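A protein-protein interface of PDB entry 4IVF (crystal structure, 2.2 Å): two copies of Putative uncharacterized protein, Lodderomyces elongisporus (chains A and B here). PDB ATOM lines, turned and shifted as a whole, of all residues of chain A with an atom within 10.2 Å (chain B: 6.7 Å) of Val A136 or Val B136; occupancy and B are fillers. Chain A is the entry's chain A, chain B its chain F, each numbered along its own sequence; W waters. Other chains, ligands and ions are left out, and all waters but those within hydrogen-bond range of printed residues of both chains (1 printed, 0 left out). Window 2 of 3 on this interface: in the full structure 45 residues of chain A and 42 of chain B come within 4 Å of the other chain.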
ATOM      1  N   GLN A 124      14.255  -1.426  18.521  1.00  0.00           N
ATOM      2  CA  GLN A 124      12.877  -1.572  18.984  1.00  0.00           C
ATOM      3  C   GLN A 124      12.302  -2.888  18.512  1.00  0.00           C
ATOM      4  O   GLN A 124      11.617  -3.581  19.263  1.00  0.00           O
ATOM      5  CB  GLN A 124      11.995  -0.430  18.483  1.00  0.00           C
ATOM      6  CG  GLN A 124      12.471   0.934  18.903  1.00  0.00           C
ATOM      7  CD  GLN A 124      12.951   0.953  20.329  1.00  0.00           C
ATOM      8  OE1 GLN A 124      12.255   0.494  21.239  1.00  0.00           O
ATOM      9  NE2 GLN A 124      14.151   1.480  20.537  1.00  0.00           N
ATOM     10  N   ALA A 125      12.594  -3.237  17.267  1.00  0.00           N
ATOM     11  CA  ALA A 125      12.182  -4.537  16.756  1.00  0.00           C
ATOM     12  C   ALA A 125      12.733  -5.656  17.643  1.00  0.00           C
ATOM     13  O   ALA A 125      12.005  -6.571  18.031  1.00  0.00           O
ATOM     14  CB  ALA A 125      12.625  -4.719  15.291  1.00  0.00           C
ATOM     15  N   HIS A 127      13.555  -5.475  20.735  1.00  0.00           N
ATOM     16  CA  HIS A 127      12.840  -5.435  22.009  1.00  0.00           C
ATOM     17  C   HIS A 127      11.463  -6.131  21.963  1.00  0.00           C
ATOM     18  O   HIS A 127      11.163  -6.991  22.785  1.00  0.00           O
ATOM     19  CB  HIS A 127      12.671  -4.005  22.509  1.00  0.00           C
ATOM     20  CG  HIS A 127      11.751  -3.905  23.683  1.00  0.00           C
ATOM     21  ND1 HIS A 127      12.136  -4.255  24.957  1.00  0.00           N
ATOM     22  CD2 HIS A 127      10.451  -3.540  23.768  1.00  0.00           C
ATOM     23  CE1 HIS A 127      11.117  -4.088  25.783  1.00  0.00           C
ATOM     24  NE2 HIS A 127      10.082  -3.655  25.086  1.00  0.00           N
ATOM     25  N   PHE A 128      10.625  -5.770  21.000  1.00  0.00           N
ATOM     26  CA  PHE A 128       9.310  -6.393  20.930  1.00  0.00           C
ATOM     27  C   PHE A 128       9.373  -7.863  20.587  1.00  0.00           C
ATOM     28  O   PHE A 128       8.518  -8.623  20.995  1.00  0.00           O
ATOM     29  CB  PHE A 128       8.388  -5.654  19.978  1.00  0.00           C
ATOM     30  CG  PHE A 128       7.882  -4.372  20.531  1.00  0.00           C
ATOM     31  CD1 PHE A 128       6.717  -4.342  21.284  1.00  0.00           C
ATOM     32  CD2 PHE A 128       8.577  -3.193  20.317  1.00  0.00           C
ATOM     33  CE1 PHE A 128       6.251  -3.157  21.807  1.00  0.00           C
ATOM     34  CE2 PHE A 128       8.113  -2.002  20.831  1.00  0.00           C
ATOM     35  CZ  PHE A 128       6.939  -1.985  21.579  1.00  0.00           C
ATOM     36  N   VAL A 129      10.398  -8.276  19.855  1.00  0.00           N
ATOM     37  CA  VAL A 129      10.513  -9.691  19.514  1.00  0.00           C
ATOM     38  C   VAL A 129      11.138 -10.536  20.631  1.00  0.00           C
ATOM     39  O   VAL A 129      10.646 -11.618  20.942  1.00  0.00           O
ATOM     40  CB  VAL A 129      11.271  -9.911  18.190  1.00  0.00           C
ATOM     41  CG1 VAL A 129      11.528 -11.403  17.966  1.00  0.00           C
ATOM     42  CG2 VAL A 129      10.485  -9.300  17.024  1.00  0.00           C
ATOM     43  N   PHE A 130      12.214 -10.051  21.243  1.00  0.00           N
ATOM     44  CA  PHE A 130      12.941 -10.885  22.208  1.00  0.00           C
ATOM     45  C   PHE A 130      12.789 -10.518  23.681  1.00  0.00           C
ATOM     46  O   PHE A 130      12.791 -11.398  24.542  1.00  0.00           O
ATOM     47  CB  PHE A 130      14.424 -10.937  21.847  1.00  0.00           C
ATOM     48  CG  PHE A 130      14.685 -11.479  20.473  1.00  0.00           C
ATOM     49  CD1 PHE A 130      14.485 -12.824  20.196  1.00  0.00           C
ATOM     50  CD2 PHE A 130      15.126 -10.649  19.460  1.00  0.00           C
ATOM     51  CE1 PHE A 130      14.723 -13.329  18.935  1.00  0.00           C
ATOM     52  CE2 PHE A 130      15.368 -11.148  18.195  1.00  0.00           C
ATOM     53  CZ  PHE A 130      15.165 -12.489  17.934  1.00  0.00           C
ATOM     54  N   ALA A 131      12.666  -9.231  23.976  1.00  0.00           N
ATOM     55  CA  ALA A 131      12.805  -8.761  25.357  1.00  0.00           C
ATOM     56  C   ALA A 131      11.490  -8.492  26.098  1.00  0.00           C
ATOM     57  O   ALA A 131      11.368  -8.822  27.272  1.00  0.00           O
ATOM     58  CB  ALA A 131      13.706  -7.526  25.404  1.00  0.00           C
ATOM     59  N   ALA A 132      10.525  -7.894  25.402  1.00  0.00           N
ATOM     60  CA  ALA A 132       9.260  -7.466  26.000  1.00  0.00           C
ATOM     61  C   ALA A 132       8.588  -8.573  26.801  1.00  0.00           C
ATOM     62  O   ALA A 132       8.498  -9.710  26.347  1.00  0.00           O
ATOM     63  CB  ALA A 132       8.316  -6.935  24.930  1.00  0.00           C
ATOM     64  N   LYS A 133       8.122  -8.229  27.997  1.00  0.00           N
ATOM     65  CA  LYS A 133       7.529  -9.221  28.897  1.00  0.00           C
ATOM     66  C   LYS A 133       6.183  -9.708  28.388  1.00  0.00           C
ATOM     67  O   LYS A 133       5.700 -10.765  28.795  1.00  0.00           O
ATOM     68  CB  LYS A 133       7.386  -8.660  30.312  1.00  0.00           C
ATOM     69  CG  LYS A 133       8.687  -8.143  30.903  1.00  0.00           C
ATOM     70  CD  LYS A 133       9.811  -9.172  30.791  1.00  0.00           C
ATOM     71  CE  LYS A 133       9.576 -10.372  31.700  1.00  0.00           C
ATOM     72  NZ  LYS A 133      10.702 -11.342  31.628  1.00  0.00           N
ATOM     73  N   GLU A 134       5.577  -8.932  27.497  1.00  0.00           N
ATOM     74  CA  GLU A 134       4.351  -9.360  26.844  1.00  0.00           C
ATOM     75  C   GLU A 134       4.475  -9.277  25.329  1.00  0.00           C
ATOM     76  O   GLU A 134       5.290  -8.513  24.791  1.00  0.00           O
ATOM     77  CB  GLU A 134       3.148  -8.551  27.333  1.00  0.00           C
ATOM     78  CG  GLU A 134       3.400  -7.063  27.452  1.00  0.00           C
ATOM     79  CD  GLU A 134       2.117  -6.277  27.644  1.00  0.00           C
ATOM     80  OE1 GLU A 134       1.239  -6.360  26.756  1.00  0.00           O
ATOM     81  OE2 GLU A 134       1.983  -5.579  28.673  1.00  0.00           O
ATOM     82  N   LYS A 135       3.673 -10.087  24.646  1.00  0.00           N
ATOM     83  CA  LYS A 135       3.624 -10.072  23.196  1.00  0.00           C
ATOM     84  C   LYS A 135       2.748  -8.912  22.759  1.00  0.00           C
ATOM     85  O   LYS A 135       1.585  -8.839  23.137  1.00  0.00           O
ATOM     86  CB  LYS A 135       3.062 -11.388  22.676  1.00  0.00           C
ATOM     87  CG  LYS A 135       3.225 -11.571  21.181  1.00  0.00           C
ATOM     88  CD  LYS A 135       2.685 -12.918  20.728  1.00  0.00           C
ATOM     89  CE  LYS A 135       2.836 -13.106  19.226  1.00  0.00           C
ATOM     90  NZ  LYS A 135       2.295 -14.422  18.805  1.00  0.00           N
ATOM     91  N   VAL A 136       3.314  -8.001  21.971  1.00  0.00           N
ATOM     92  CA  VAL A 136       2.579  -6.840  21.467  1.00  0.00           C
ATOM     93  C   VAL A 136       2.713  -6.759  19.944  1.00  0.00           C
ATOM     94  O   VAL A 136       3.645  -6.128  19.445  1.00  0.00           O
ATOM     95  CB  VAL A 136       3.136  -5.519  22.068  1.00  0.00           C
ATOM     96  CG1 VAL A 136       2.237  -4.353  21.718  1.00  0.00           C
ATOM     97  CG2 VAL A 136       3.317  -5.622  23.570  1.00  0.00           C
ATOM     98  N   PRO A 137       1.791  -7.406  19.198  1.00  0.00           N
ATOM     99  CA  PRO A 137       1.886  -7.531  17.728  1.00  0.00           C
ATOM    100  C   PRO A 137       2.007  -6.192  17.016  1.00  0.00           C
ATOM    101  O   PRO A 137       2.772  -6.082  16.047  1.00  0.00           O
ATOM    102  CB  PRO A 137       0.563  -8.220  17.331  1.00  0.00           C
ATOM    103  CG  PRO A 137       0.167  -8.982  18.548  1.00  0.00           C
ATOM    104  CD  PRO A 137       0.629  -8.130  19.738  1.00  0.00           C
ATOM    105  N   TYR A 138       1.260  -5.195  17.486  1.00  0.00           N
ATOM    106  CA  TYR A 138       1.345  -3.870  16.904  1.00  0.00           C
ATOM    107  C   TYR A 138       2.795  -3.400  16.841  1.00  0.00           C
ATOM    108  O   TYR A 138       3.246  -2.906  15.807  1.00  0.00           O
ATOM    109  CB  TYR A 138       0.478  -2.868  17.666  1.00  0.00           C
ATOM    110  CG  TYR A 138       0.449  -1.513  16.998  1.00  0.00           C
ATOM    111  CD1 TYR A 138       1.446  -0.568  17.255  1.00  0.00           C
ATOM    112  CD2 TYR A 138      -0.561  -1.178  16.094  1.00  0.00           C
ATOM    113  CE1 TYR A 138       1.439   0.679  16.636  1.00  0.00           C
ATOM    114  CE2 TYR A 138      -0.582   0.072  15.468  1.00  0.00           C
ATOM    115  CZ  TYR A 138       0.428   0.996  15.747  1.00  0.00           C
ATOM    116  OH  TYR A 138       0.435   2.239  15.149  1.00  0.00           O
ATOM    117  N   GLY A 139       3.528  -3.581  17.941  1.00  0.00           N
ATOM    118  CA  GLY A 139       4.903  -3.123  18.022  1.00  0.00           C
ATOM    119  C   GLY A 139       5.857  -3.975  17.192  1.00  0.00           C
ATOM    120  O   GLY A 139       6.753  -3.459  16.521  1.00  0.00           O
ATOM    121  N   ILE A 140       5.656  -5.287  17.248  1.00  0.00           N
ATOM    122  CA  ILE A 140       6.433  -6.227  16.468  1.00  0.00           C
ATOM    123  C   ILE A 140       6.275  -5.895  14.998  1.00  0.00           C
ATOM    124  O   ILE A 140       7.257  -5.808  14.262  1.00  0.00           O
ATOM    125  CB  ILE A 140       5.941  -7.663  16.717  1.00  0.00           C
ATOM    126  CG1 ILE A 140       6.121  -8.020  18.201  1.00  0.00           C
ATOM    127  CG2 ILE A 140       6.662  -8.645  15.802  1.00  0.00           C
ATOM    128  CD1 ILE A 140       5.825  -9.480  18.546  1.00  0.00           C
ATOM    129  N   ASN A 141       5.032  -5.683  14.579  1.00  0.00           N
ATOM    130  CA  ASN A 141       4.764  -5.323  13.202  1.00  0.00           C
ATOM    131  C   ASN A 141       5.297  -3.950  12.810  1.00  0.00           C
ATOM    132  O   ASN A 141       5.907  -3.807  11.763  1.00  0.00           O
ATOM    133  CB  ASN A 141       3.269  -5.451  12.871  1.00  0.00           C
ATOM    134  CG  ASN A 141       2.957  -5.067  11.438  1.00  0.00           C
ATOM    135  OD1 ASN A 141       3.133  -5.868  10.515  1.00  0.00           O
ATOM    136  ND2 ASN A 141       2.498  -3.836  11.241  1.00  0.00           N
ATOM    137  N   ARG A 142       5.086  -2.943  13.642  1.00  0.00           N
ATOM    138  CA  ARG A 142       5.574  -1.601  13.315  1.00  0.00           C
ATOM    139  C   ARG A 142       7.094  -1.548  13.097  1.00  0.00           C
ATOM    140  O   ARG A 142       7.570  -0.910  12.156  1.00  0.00           O
ATOM    141  CB  ARG A 142       5.144  -0.586  14.381  1.00  0.00           C
ATOM    142  CG  ARG A 142       5.837   0.772  14.278  1.00  0.00           C
ATOM    143  CD  ARG A 142       5.277   1.768  15.290  1.00  0.00           C
ATOM    144  NE  ARG A 142       6.022   3.030  15.312  1.00  0.00           N
ATOM    145  CZ  ARG A 142       5.794   4.033  14.471  1.00  0.00           C
ATOM    146  NH1 ARG A 142       4.855   3.903  13.547  1.00  0.00           N
ATOM    147  NH2 ARG A 142       6.509   5.153  14.538  1.00  0.00           N
ATOM    148  N   TYR A 143       7.853  -2.231  13.945  1.00  0.00           N
ATOM    149  CA  TYR A 143       9.311  -2.110  13.892  1.00  0.00           C
ATOM    150  C   TYR A 143       9.999  -3.104  12.942  1.00  0.00           C
ATOM    151  O   TYR A 143      11.030  -2.788  12.354  1.00  0.00           O
ATOM    152  CB  TYR A 143       9.923  -2.079  15.313  1.00  0.00           C
ATOM    153  CG  TYR A 143       9.374  -0.905  16.088  1.00  0.00           C
ATOM    154  CD1 TYR A 143       9.782   0.390  15.794  1.00  0.00           C
ATOM    155  CD2 TYR A 143       8.411  -1.079  17.074  1.00  0.00           C
ATOM    156  CE1 TYR A 143       9.256   1.474  16.465  1.00  0.00           C
ATOM    157  CE2 TYR A 143       7.871   0.007  17.753  1.00  0.00           C
ATOM    158  CZ  TYR A 143       8.295   1.275  17.433  1.00  0.00           C
ATOM    159  OH  TYR A 143       7.780   2.362  18.096  1.00  0.00           O
ATOM    160  N   ILE A 144       9.417  -4.282  12.760  1.00  0.00           N
ATOM    161  CA  ILE A 144       9.891  -5.175  11.705  1.00  0.00           C
ATOM    162  C   ILE A 144       9.719  -4.486  10.350  1.00  0.00           C
ATOM    163  O   ILE A 144      10.626  -4.483   9.514  1.00  0.00           O
ATOM    164  CB  ILE A 144       9.150  -6.517  11.701  1.00  0.00           C
ATOM    165  CG1 ILE A 144       9.608  -7.374  12.882  1.00  0.00           C
ATOM    166  CG2 ILE A 144       9.401  -7.262  10.391  1.00  0.00           C
ATOM    167  CD1 ILE A 144      11.068  -7.666  12.864  1.00  0.00           C
ATOM    168  N   PHE B 128       2.575   6.786  19.469  1.00  0.00           N
ATOM    169  CA  PHE B 128       1.649   5.952  20.236  1.00  0.00           C
ATOM    170  C   PHE B 128       0.503   6.731  20.859  1.00  0.00           C
ATOM    171  O   PHE B 128      -0.552   6.177  21.162  1.00  0.00           O
ATOM    172  CB  PHE B 128       2.387   5.093  21.265  1.00  0.00           C
ATOM    173  CG  PHE B 128       3.021   3.872  20.661  1.00  0.00           C
ATOM    174  CD1 PHE B 128       2.271   2.722  20.445  1.00  0.00           C
ATOM    175  CD2 PHE B 128       4.348   3.883  20.264  1.00  0.00           C
ATOM    176  CE1 PHE B 128       2.836   1.600  19.869  1.00  0.00           C
ATOM    177  CE2 PHE B 128       4.924   2.760  19.680  1.00  0.00           C
ATOM    178  CZ  PHE B 128       4.161   1.614  19.486  1.00  0.00           C
ATOM    179  N   ALA B 132      -1.155   6.361  16.286  1.00  0.00           N
ATOM    180  CA  ALA B 132      -1.557   4.958  16.217  1.00  0.00           C
ATOM    181  C   ALA B 132      -3.077   4.801  16.094  1.00  0.00           C
ATOM    182  O   ALA B 132      -3.841   5.553  16.707  1.00  0.00           O
ATOM    183  CB  ALA B 132      -1.026   4.177  17.412  1.00  0.00           C
ATOM    184  N   GLU B 134      -4.782   2.241  17.012  1.00  0.00           N
ATOM    185  CA  GLU B 134      -5.328   1.620  18.206  1.00  0.00           C
ATOM    186  C   GLU B 134      -4.563   2.113  19.428  1.00  0.00           C
ATOM    187  O   GLU B 134      -3.474   2.686  19.305  1.00  0.00           O
ATOM    188  CB  GLU B 134      -5.299   0.090  18.098  1.00  0.00           C
ATOM    189  CG  GLU B 134      -3.914  -0.523  18.103  1.00  0.00           C
ATOM    190  CD  GLU B 134      -3.900  -1.937  17.553  1.00  0.00           C
ATOM    191  OE1 GLU B 134      -3.656  -2.891  18.326  1.00  0.00           O
ATOM    192  OE2 GLU B 134      -4.133  -2.089  16.336  1.00  0.00           O
ATOM    193  N   LYS B 135      -5.152   1.926  20.604  1.00  0.00           N
ATOM    194  CA  LYS B 135      -4.479   2.294  21.833  1.00  0.00           C
ATOM    195  C   LYS B 135      -3.578   1.143  22.240  1.00  0.00           C
ATOM    196  O   LYS B 135      -4.053   0.045  22.502  1.00  0.00           O
ATOM    197  CB  LYS B 135      -5.485   2.610  22.949  1.00  0.00           C
ATOM    198  CG  LYS B 135      -4.818   3.117  24.234  1.00  0.00           C
ATOM    199  CD  LYS B 135      -5.822   3.429  25.348  1.00  0.00           C
ATOM    200  CE  LYS B 135      -6.369   2.163  25.973  1.00  0.00           C
ATOM    201  NZ  LYS B 135      -7.178   2.454  27.193  1.00  0.00           N
ATOM    202  N   VAL B 136      -2.275   1.390  22.276  1.00  0.00           N
ATOM    203  CA  VAL B 136      -1.333   0.373  22.723  1.00  0.00           C
ATOM    204  C   VAL B 136      -0.610   0.883  23.979  1.00  0.00           C
ATOM    205  O   VAL B 136       0.428   1.545  23.894  1.00  0.00           O
ATOM    206  CB  VAL B 136      -0.325  -0.017  21.602  1.00  0.00           C
ATOM    207  CG1 VAL B 136       0.322  -1.349  21.911  1.00  0.00           C
ATOM    208  CG2 VAL B 136      -1.028  -0.095  20.254  1.00  0.00           C
ATOM    209  N   PRO B 137      -1.178   0.596  25.157  1.00  0.00           N
ATOM    210  CA  PRO B 137      -0.648   1.103  26.429  1.00  0.00           C
ATOM    211  C   PRO B 137       0.827   0.756  26.658  1.00  0.00           C
ATOM    212  O   PRO B 137       1.564   1.592  27.177  1.00  0.00           O
ATOM    213  CB  PRO B 137      -1.524   0.411  27.469  1.00  0.00           C
ATOM    214  CG  PRO B 137      -2.823   0.173  26.758  1.00  0.00           C
ATOM    215  CD  PRO B 137      -2.435  -0.152  25.340  1.00  0.00           C
ATOM    216  N   TYR B 138       1.243  -0.454  26.286  1.00  0.00           N
ATOM    217  CA  TYR B 138       2.632  -0.862  26.442  1.00  0.00           C
ATOM    218  C   TYR B 138       3.538   0.127  25.731  1.00  0.00           C
ATOM    219  O   TYR B 138       4.595   0.500  26.245  1.00  0.00           O
ATOM    220  CB  TYR B 138       2.864  -2.269  25.892  1.00  0.00           C
ATOM    221  CG  TYR B 138       4.268  -2.783  26.134  1.00  0.00           C
ATOM    222  CD1 TYR B 138       5.307  -2.456  25.269  1.00  0.00           C
ATOM    223  CD2 TYR B 138       4.557  -3.590  27.226  1.00  0.00           C
ATOM    224  CE1 TYR B 138       6.593  -2.910  25.483  1.00  0.00           C
ATOM    225  CE2 TYR B 138       5.840  -4.053  27.446  1.00  0.00           C
ATOM    226  CZ  TYR B 138       6.855  -3.709  26.570  1.00  0.00           C
ATOM    227  OH  TYR B 138       8.139  -4.163  26.772  1.00  0.00           O
ATOM    228  N   GLY B 139       3.104   0.556  24.549  1.00  0.00           N
ATOM    229  CA  GLY B 139       3.875   1.484  23.745  1.00  0.00           C
ATOM    230  C   GLY B 139       3.897   2.874  24.349  1.00  0.00           C
ATOM    231  O   GLY B 139       4.950   3.491  24.465  1.00  0.00           O
ATOM    232  N   ILE B 140       2.719   3.374  24.697  1.00  0.00           N
ATOM    233  CA  ILE B 140       2.594   4.680  25.320  1.00  0.00           C
ATOM    234  C   ILE B 140       3.495   4.775  26.554  1.00  0.00           C
ATOM    235  O   ILE B 140       4.261   5.721  26.691  1.00  0.00           O
ATOM    236  CB  ILE B 140       1.145   4.962  25.741  1.00  0.00           C
ATOM    237  CG1 ILE B 140       0.242   5.123  24.513  1.00  0.00           C
ATOM    238  CG2 ILE B 140       1.075   6.186  26.638  1.00  0.00           C
ATOM    239  CD1 ILE B 140      -1.255   5.113  24.874  1.00  0.00           C
ATOM    240  N   ASN B 141       3.412   3.783  27.430  1.00  0.00           N
ATOM    241  CA  ASN B 141       4.192   3.798  28.659  1.00  0.00           C
ATOM    242  C   ASN B 141       5.683   3.680  28.389  1.00  0.00           C
ATOM    243  O   ASN B 141       6.477   4.405  28.988  1.00  0.00           O
ATOM    244  CB  ASN B 141       3.758   2.675  29.614  1.00  0.00           C
ATOM    245  CG  ASN B 141       2.339   2.847  30.117  1.00  0.00           C
ATOM    246  OD1 ASN B 141       1.812   3.957  30.166  1.00  0.00           O
ATOM    247  ND2 ASN B 141       1.715   1.737  30.506  1.00  0.00           N
HETATM  248  O   HOH W   1       8.800  -5.448  29.078  1.00  0.00           O
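Among the printed residues, merely in contact across the chains: Phe A128 with Tyr B138 (3.7 Å), Ala A132 with Tyr B138 (3.3 Å), Glu A134 with Tyr B138 (3.6 Å), Val A136 with Val B136 (3.6 Å), Val A136 with Tyr B138 (3.9 Å), Tyr A138 with Phe B128 (3.6 Å), Tyr A138 with Ala B132 (3.3 Å), Tyr A138 with Glu B134 (3.7 Å), Tyr A138 with Val B136 (3.8 Å) and Tyr A143 with Phe B128 (3.3 Å).
Of the 20 printed residues of chain A, 7 touch a printed residue of chain B.
Hydrophobic or aromatic side chains of chain A that line the printed part of chain B: His A127, Phe A128, Ala A132, Val A136, Tyr A138 and Tyr A143.
Of the 10 printed residues of chain B, 5 touch a printed residue of chain A.
Hydrophobic or aromatic side chains of chain B that line the printed part of chain A: Phe B128, Ala B132, Val B136 and Tyr B138.
N of Ala A132 sits at hydrogen-bond distance from O of His A127, 2.8 Å away.
The guanidinium group (NE) of Arg A142 lies within hydrogen-bond range of the side-chain hydroxyl (OH) of Tyr A143 (3.4 Å).
Water W1 lies within hydrogen-bond range of OH of Tyr B138 and N of Lys A133.
Gln A124 touches none of the printed residues of chain B.
Printed residues of chain B within 4 Å of Glu A134: Tyr B138.
Of chain B, only Val B136 and Tyr B138 come within 4 Å of Val A136.
Of the printed residues of chain B, Tyr A138 touches Phe B128, Ala B132, Glu B134 and Val B136.
Of the printed residues of chain A, Phe B128 touches Tyr A138 and Tyr A143.
Printed residues of chain A within 4 Å of Ala B132: Tyr A138.
Of chain A, only Tyr A138 comes within 4 Å of Glu B134.
Val B136 touches just these residues of chain A: Val A136 and Tyr A138.
No residue of chain A comes within 4 Å of Pro B137.
No residue of chain A comes within 4 Å of Gly B139.
OH of Tyr B138 sits at hydrogen-bond distance from NE2 of His A127.
Phe A128 touches Tyr B138, and with the chains exchanged Tyr A138 touches Phe B128.
Ala A132 touches Tyr B138, and with the chains exchanged Tyr A138 touches Ala B132.
Val A136 touches its own counterpart, Val B136.
Val A136 touches Tyr B138, and with the chains exchanged Tyr A138 touches Val B136.
Positions printed for both chains: 128, 132, 134, 135, 136, 137, 138, 139, 140 and 141.
Of the 11 pairs that touch across the chains among the printed residues, 9 have their exchanged pair printed and touching as well.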
